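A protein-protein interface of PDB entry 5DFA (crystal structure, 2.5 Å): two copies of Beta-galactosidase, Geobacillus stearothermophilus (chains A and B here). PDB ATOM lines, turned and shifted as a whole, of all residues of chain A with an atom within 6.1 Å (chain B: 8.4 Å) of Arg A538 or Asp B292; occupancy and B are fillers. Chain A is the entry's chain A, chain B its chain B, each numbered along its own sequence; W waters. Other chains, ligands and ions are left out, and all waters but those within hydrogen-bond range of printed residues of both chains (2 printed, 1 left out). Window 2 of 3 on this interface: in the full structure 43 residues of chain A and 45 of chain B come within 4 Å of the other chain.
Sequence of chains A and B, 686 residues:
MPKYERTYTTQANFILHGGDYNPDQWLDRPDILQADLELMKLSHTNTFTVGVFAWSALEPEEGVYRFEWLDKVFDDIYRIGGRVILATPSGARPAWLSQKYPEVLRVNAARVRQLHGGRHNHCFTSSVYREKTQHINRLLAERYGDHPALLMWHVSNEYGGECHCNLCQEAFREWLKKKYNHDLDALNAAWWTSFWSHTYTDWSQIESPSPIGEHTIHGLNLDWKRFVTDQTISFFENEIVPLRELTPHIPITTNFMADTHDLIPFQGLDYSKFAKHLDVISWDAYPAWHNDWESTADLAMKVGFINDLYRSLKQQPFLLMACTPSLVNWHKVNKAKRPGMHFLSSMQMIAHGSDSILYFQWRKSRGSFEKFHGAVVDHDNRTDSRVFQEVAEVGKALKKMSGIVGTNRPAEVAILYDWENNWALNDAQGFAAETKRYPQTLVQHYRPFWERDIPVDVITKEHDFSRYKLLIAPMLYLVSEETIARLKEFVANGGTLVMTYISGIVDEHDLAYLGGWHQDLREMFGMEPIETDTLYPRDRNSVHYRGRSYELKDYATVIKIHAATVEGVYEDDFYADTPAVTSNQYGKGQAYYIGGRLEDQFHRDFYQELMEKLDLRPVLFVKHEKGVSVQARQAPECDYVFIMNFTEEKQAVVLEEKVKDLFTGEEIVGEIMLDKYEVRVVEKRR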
ATOM      1  N   TYR A 536      -9.319 -21.998 -11.457  1.00  0.00           N
ATOM      2  CA  TYR A 536      -8.067 -22.089 -12.197  1.00  0.00           C
ATOM      3  C   TYR A 536      -7.460 -20.689 -12.343  1.00  0.00           C
ATOM      4  O   TYR A 536      -8.167 -19.698 -12.156  1.00  0.00           O
ATOM      5  CB  TYR A 536      -8.311 -22.744 -13.562  1.00  0.00           C
ATOM      6  CG  TYR A 536      -8.482 -24.245 -13.489  1.00  0.00           C
ATOM      7  CD1 TYR A 536      -9.720 -24.810 -13.205  1.00  0.00           C
ATOM      8  CD2 TYR A 536      -7.406 -25.098 -13.701  1.00  0.00           C
ATOM      9  CE1 TYR A 536      -9.881 -26.182 -13.133  1.00  0.00           C
ATOM     10  CE2 TYR A 536      -7.558 -26.472 -13.634  1.00  0.00           C
ATOM     11  CZ  TYR A 536      -8.798 -27.008 -13.350  1.00  0.00           C
ATOM     12  OH  TYR A 536      -8.953 -28.374 -13.281  1.00  0.00           O
ATOM     13  N   PRO A 537      -6.152 -20.600 -12.656  1.00  0.00           N
ATOM     14  CA  PRO A 537      -5.475 -19.297 -12.734  1.00  0.00           C
ATOM     15  C   PRO A 537      -6.150 -18.272 -13.648  1.00  0.00           C
ATOM     16  O   PRO A 537      -6.109 -17.078 -13.351  1.00  0.00           O
ATOM     17  CB  PRO A 537      -4.092 -19.659 -13.278  1.00  0.00           C
ATOM     18  CG  PRO A 537      -3.861 -21.041 -12.802  1.00  0.00           C
ATOM     19  CD  PRO A 537      -5.203 -21.714 -12.842  1.00  0.00           C
ATOM     20  N   ARG A 538      -6.763 -18.729 -14.735  1.00  0.00           N
ATOM     21  CA  ARG A 538      -7.363 -17.819 -15.705  1.00  0.00           C
ATOM     22  C   ARG A 538      -8.828 -17.518 -15.390  1.00  0.00           C
ATOM     23  O   ARG A 538      -9.429 -16.632 -15.998  1.00  0.00           O
ATOM     24  CB  ARG A 538      -7.229 -18.393 -17.117  1.00  0.00           C
ATOM     25  CG  ARG A 538      -5.787 -18.475 -17.601  1.00  0.00           C
ATOM     26  CD  ARG A 538      -5.636 -19.379 -18.816  1.00  0.00           C
ATOM     27  NE  ARG A 538      -5.911 -18.682 -20.069  1.00  0.00           N
ATOM     28  CZ  ARG A 538      -7.004 -18.862 -20.802  1.00  0.00           C
ATOM     29  NH1 ARG A 538      -7.934 -19.724 -20.411  1.00  0.00           N
ATOM     30  NH2 ARG A 538      -7.167 -18.183 -21.929  1.00  0.00           N
ATOM     31  N   ASP A 539      -9.399 -18.255 -14.440  1.00  0.00           N
ATOM     32  CA  ASP A 539     -10.777 -18.019 -14.019  1.00  0.00           C
ATOM     33  C   ASP A 539     -10.916 -16.672 -13.319  1.00  0.00           C
ATOM     34  O   ASP A 539     -10.052 -16.274 -12.537  1.00  0.00           O
ATOM     35  CB  ASP A 539     -11.263 -19.135 -13.090  1.00  0.00           C
ATOM     36  CG  ASP A 539     -11.455 -20.454 -13.808  1.00  0.00           C
ATOM     37  OD1 ASP A 539     -11.665 -20.438 -15.039  1.00  0.00           O
ATOM     38  OD2 ASP A 539     -11.401 -21.507 -13.139  1.00  0.00           O
ATOM     39  N   ARG A 540     -12.011 -15.976 -13.605  1.00  0.00           N
ATOM     40  CA  ARG A 540     -12.277 -14.685 -12.986  1.00  0.00           C
ATOM     41  C   ARG A 540     -13.732 -14.555 -12.563  1.00  0.00           C
ATOM     42  O   ARG A 540     -14.625 -15.149 -13.167  1.00  0.00           O
ATOM     43  CB  ARG A 540     -11.922 -13.540 -13.941  1.00  0.00           C
ATOM     44  CG  ARG A 540     -10.441 -13.392 -14.238  1.00  0.00           C
ATOM     45  CD  ARG A 540      -9.671 -12.915 -13.016  1.00  0.00           C
ATOM     46  NE  ARG A 540      -8.259 -12.700 -13.320  1.00  0.00           N
ATOM     47  CZ  ARG A 540      -7.338 -13.659 -13.309  1.00  0.00           C
ATOM     48  NH1 ARG A 540      -7.677 -14.905 -13.007  1.00  0.00           N
ATOM     49  NH2 ARG A 540      -6.076 -13.371 -13.598  1.00  0.00           N
ATOM     50  N   ALA B 288     -10.828 -33.452 -15.761  1.00  0.00           N
ATOM     51  CA  ALA B 288     -10.727 -32.151 -15.116  1.00  0.00           C
ATOM     52  C   ALA B 288     -11.637 -31.143 -15.805  1.00  0.00           C
ATOM     53  O   ALA B 288     -11.164 -30.253 -16.513  1.00  0.00           O
ATOM     54  CB  ALA B 288      -9.289 -31.662 -15.125  1.00  0.00           C
ATOM     55  N   TRP B 289     -12.944 -31.292 -15.600  1.00  0.00           N
ATOM     56  CA  TRP B 289     -13.923 -30.407 -16.220  1.00  0.00           C
ATOM     57  C   TRP B 289     -13.693 -28.955 -15.813  1.00  0.00           C
ATOM     58  O   TRP B 289     -13.250 -28.677 -14.697  1.00  0.00           O
ATOM     59  CB  TRP B 289     -15.351 -30.829 -15.855  1.00  0.00           C
ATOM     60  CG  TRP B 289     -15.735 -32.204 -16.332  1.00  0.00           C
ATOM     61  CD1 TRP B 289     -15.934 -33.312 -15.562  1.00  0.00           C
ATOM     62  CD2 TRP B 289     -15.969 -32.610 -17.688  1.00  0.00           C
ATOM     63  NE1 TRP B 289     -16.278 -34.383 -16.351  1.00  0.00           N
ATOM     64  CE2 TRP B 289     -16.305 -33.980 -17.660  1.00  0.00           C
ATOM     65  CE3 TRP B 289     -15.927 -31.951 -18.921  1.00  0.00           C
ATOM     66  CZ2 TRP B 289     -16.595 -34.701 -18.817  1.00  0.00           C
ATOM     67  CZ3 TRP B 289     -16.216 -32.670 -20.069  1.00  0.00           C
ATOM     68  CH2 TRP B 289     -16.546 -34.030 -20.008  1.00  0.00           C
ATOM     69  N   HIS B 290     -13.983 -28.045 -16.740  1.00  0.00           N
ATOM     70  CA  HIS B 290     -13.884 -26.602 -16.522  1.00  0.00           C
ATOM     71  C   HIS B 290     -12.459 -26.126 -16.244  1.00  0.00           C
ATOM     72  O   HIS B 290     -12.262 -25.107 -15.582  1.00  0.00           O
ATOM     73  CB  HIS B 290     -14.801 -26.166 -15.373  1.00  0.00           C
ATOM     74  CG  HIS B 290     -16.131 -26.850 -15.368  1.00  0.00           C
ATOM     75  ND1 HIS B 290     -16.998 -26.800 -16.438  1.00  0.00           N
ATOM     76  CD2 HIS B 290     -16.741 -27.606 -14.424  1.00  0.00           C
ATOM     77  CE1 HIS B 290     -18.086 -27.494 -16.153  1.00  0.00           C
ATOM     78  NE2 HIS B 290     -17.954 -27.994 -14.937  1.00  0.00           N
ATOM     79  N   ASN B 291     -11.467 -26.853 -16.751  1.00  0.00           N
ATOM     80  CA  ASN B 291     -10.088 -26.385 -16.668  1.00  0.00           C
ATOM     81  C   ASN B 291      -9.868 -25.248 -17.661  1.00  0.00           C
ATOM     82  O   ASN B 291     -10.736 -24.966 -18.488  1.00  0.00           O
ATOM     83  CB  ASN B 291      -9.097 -27.527 -16.917  1.00  0.00           C
ATOM     84  CG  ASN B 291      -9.172 -28.074 -18.330  1.00  0.00           C
ATOM     85  OD1 ASN B 291      -8.720 -27.436 -19.281  1.00  0.00           O
ATOM     86  ND2 ASN B 291      -9.734 -29.268 -18.471  1.00  0.00           N
ATOM     87  N   ASP B 292      -8.711 -24.598 -17.588  1.00  0.00           N
ATOM     88  CA  ASP B 292      -8.472 -23.404 -18.392  1.00  0.00           C
ATOM     89  C   ASP B 292      -7.386 -23.585 -19.452  1.00  0.00           C
ATOM     90  O   ASP B 292      -6.736 -22.618 -19.844  1.00  0.00           O
ATOM     91  CB  ASP B 292      -8.106 -22.227 -17.484  1.00  0.00           C
ATOM     92  CG  ASP B 292      -6.798 -22.442 -16.744  1.00  0.00           C
ATOM     93  OD1 ASP B 292      -6.380 -23.610 -16.596  1.00  0.00           O
ATOM     94  OD2 ASP B 292      -6.189 -21.443 -16.309  1.00  0.00           O
ATOM     95  N   TRP B 293      -7.191 -24.815 -19.919  1.00  0.00           N
ATOM     96  CA  TRP B 293      -6.189 -25.066 -20.951  1.00  0.00           C
ATOM     97  C   TRP B 293      -6.786 -25.742 -22.183  1.00  0.00           C
ATOM     98  O   TRP B 293      -6.091 -25.965 -23.175  1.00  0.00           O
ATOM     99  CB  TRP B 293      -5.038 -25.911 -20.393  1.00  0.00           C
ATOM    100  CG  TRP B 293      -5.431 -27.278 -19.906  1.00  0.00           C
ATOM    101  CD1 TRP B 293      -5.775 -28.356 -20.670  1.00  0.00           C
ATOM    102  CD2 TRP B 293      -5.493 -27.717 -18.543  1.00  0.00           C
ATOM    103  NE1 TRP B 293      -6.060 -29.435 -19.868  1.00  0.00           N
ATOM    104  CE2 TRP B 293      -5.894 -29.070 -18.558  1.00  0.00           C
ATOM    105  CE3 TRP B 293      -5.256 -27.098 -17.311  1.00  0.00           C
ATOM    106  CZ2 TRP B 293      -6.061 -29.812 -17.390  1.00  0.00           C
ATOM    107  CZ3 TRP B 293      -5.423 -27.837 -16.154  1.00  0.00           C
ATOM    108  CH2 TRP B 293      -5.821 -29.180 -16.202  1.00  0.00           C
ATOM    109  N   GLU B 294      -8.073 -26.065 -22.116  1.00  0.00           N
ATOM    110  CA  GLU B 294      -8.764 -26.690 -23.238  1.00  0.00           C
ATOM    111  C   GLU B 294     -10.266 -26.453 -23.144  1.00  0.00           C
ATOM    112  O   GLU B 294     -10.792 -26.177 -22.066  1.00  0.00           O
ATOM    113  CB  GLU B 294      -8.469 -28.192 -23.287  1.00  0.00           C
ATOM    114  CG  GLU B 294      -9.030 -28.971 -22.108  1.00  0.00           C
ATOM    115  CD  GLU B 294      -8.625 -30.432 -22.123  1.00  0.00           C
ATOM    116  OE1 GLU B 294      -8.166 -30.914 -23.180  1.00  0.00           O
ATOM    117  OE2 GLU B 294      -8.767 -31.100 -21.076  1.00  0.00           O
ATOM    118  N   SER B 295     -10.952 -26.562 -24.275  1.00  0.00           N
ATOM    119  CA  SER B 295     -12.401 -26.412 -24.296  1.00  0.00           C
ATOM    120  C   SER B 295     -13.071 -27.642 -23.700  1.00  0.00           C
ATOM    121  O   SER B 295     -12.465 -28.713 -23.621  1.00  0.00           O
ATOM    122  CB  SER B 295     -12.903 -26.178 -25.722  1.00  0.00           C
ATOM    123  OG  SER B 295     -12.811 -27.363 -26.496  1.00  0.00           O
ATOM    124  N   VAL B 333      -5.917 -28.301  -9.292  1.00  0.00           N
ATOM    125  CA  VAL B 333      -7.022 -27.389  -9.027  1.00  0.00           C
ATOM    126  C   VAL B 333      -8.321 -28.184  -8.954  1.00  0.00           C
ATOM    127  O   VAL B 333      -8.862 -28.599  -9.979  1.00  0.00           O
ATOM    128  CB  VAL B 333      -7.144 -26.299 -10.110  1.00  0.00           C
ATOM    129  CG1 VAL B 333      -8.331 -25.393  -9.819  1.00  0.00           C
ATOM    130  CG2 VAL B 333      -5.858 -25.489 -10.205  1.00  0.00           C
ATOM    131  N   LYS B 335     -11.690 -28.243  -8.962  1.00  0.00           N
ATOM    132  CA  LYS B 335     -12.883 -27.482  -9.307  1.00  0.00           C
ATOM    133  C   LYS B 335     -14.064 -28.421  -9.528  1.00  0.00           C
ATOM    134  O   LYS B 335     -13.928 -29.457 -10.179  1.00  0.00           O
ATOM    135  CB  LYS B 335     -12.616 -26.638 -10.555  1.00  0.00           C
ATOM    136  CG  LYS B 335     -13.727 -25.682 -10.946  1.00  0.00           C
ATOM    137  CD  LYS B 335     -13.257 -24.789 -12.084  1.00  0.00           C
ATOM    138  CE  LYS B 335     -14.357 -23.872 -12.581  1.00  0.00           C
ATOM    139  NZ  LYS B 335     -13.895 -23.057 -13.740  1.00  0.00           N
HETATM  140  O   HOH W   1      -6.270 -29.597 -12.247  1.00  0.00           O
HETATM  141  O   HOH W   2     -11.232 -29.472 -13.063  1.00  0.00           O
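The backbone carbonyl oxygen (O) of Val B333 lies within hydrogen-bond range of the side-chain hydroxyl (OH) of Tyr A536, at 3.3 Å. O of Asp B292 lies within hydrogen-bond range of NH1 of Arg A538 (3.2 Å). The side-chain carboxylate (OD2) of Asp A539 is in salt-bridge range of the side-chain amino group (NZ) of Lys B335 (3.0 Å).
The backbone NH (N) of Tyr A536 is in hydrogen-bond range of the side-chain carboxylate (OD2) of Asp A539. The side-chain amide nitrogen of Asn B291 lies within hydrogen-bond range of the backbone carbonyl oxygen of Ala B288. The backbone carbonyl oxygen (O) of His B290 is in hydrogen-bond range of the side-chain amino group (NZ) of Lys B335. N of Trp B293 lies within hydrogen-bond range of OD1 of Asn B291. The side-chain amide oxygen of Asn B291 lies within hydrogen-bond range of the backbone NH of Glu B294, at 3.2 Å. NE1 of Trp B293 sits at hydrogen-bond distance from OE2 of Glu B294 (3.4 Å).
Tyr A536 touches Ala B288 (OH to CB, 3.8 Å). His B290 touches Tyr A536 (O to CD1, 3.5 Å). CE1 of Tyr A536 touches CA of Asn B291, 3.5 Å away. Asp B292 touches Tyr A536 (OD1 to CD2, 3.4 Å). Trp B293 touches Tyr A536 (CZ3 to CE2, 3.6 Å). Tyr A536 touches Lys B335 (CD1 to CD, 3.7 Å). Pro A537 touches Asp B292.
Arg A538 touches one residue of chain B. Asp B292 touches just these residues of chain A: Tyr A536, Pro A537 and Arg A538. Pro A537 touches just one residue of chain B: Asp B292 (3.6 Å). Of the printed residues of chain A, Asn B291 touches Tyr A536. Of the printed residues of chain B, Tyr A536 touches Ala B288, His B290, Asn B291, Asp B292, Trp B293, Val B333 and Lys B335. Of the printed residues of chain A, Lys B335 touches Tyr A536 and Asp A539. Of the printed residues of chain B, Asp A539 touches Lys B335. The nearest residue of chain A that does not touch Asp B292 is Asp A539 (4.7 Å).
Hydrophobic or aromatic side chains of chain B within 4 Å of the printed part of chain A: Ala B288, Trp B293 and Val B333. Printed residues of chain A that touch a printed residue of chain B: Tyr A536, Pro A537, Arg A538 and Asp A539. Hydrophobic or aromatic side chains of chain A that line the printed part of chain B: Tyr A536 and Pro A537. Among the printed residues, 10 pairs touch across the chains. Among the printed residues, Asp or Glu carboxylates within 4 Å of a Lys or Arg side-chain nitrogen of the other chain: Asp A539 with Lys B335 (3.0 Å).
No position is printed for both chains.
Water W2 bridges the side-chain hydroxyl (OH) of Tyr A536 and the backbone carbonyl oxygen (O) of Trp B289. Water W1 bridges OH of Tyr A536 (3.1 Å) and N of Val B333 (3.2 Å).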
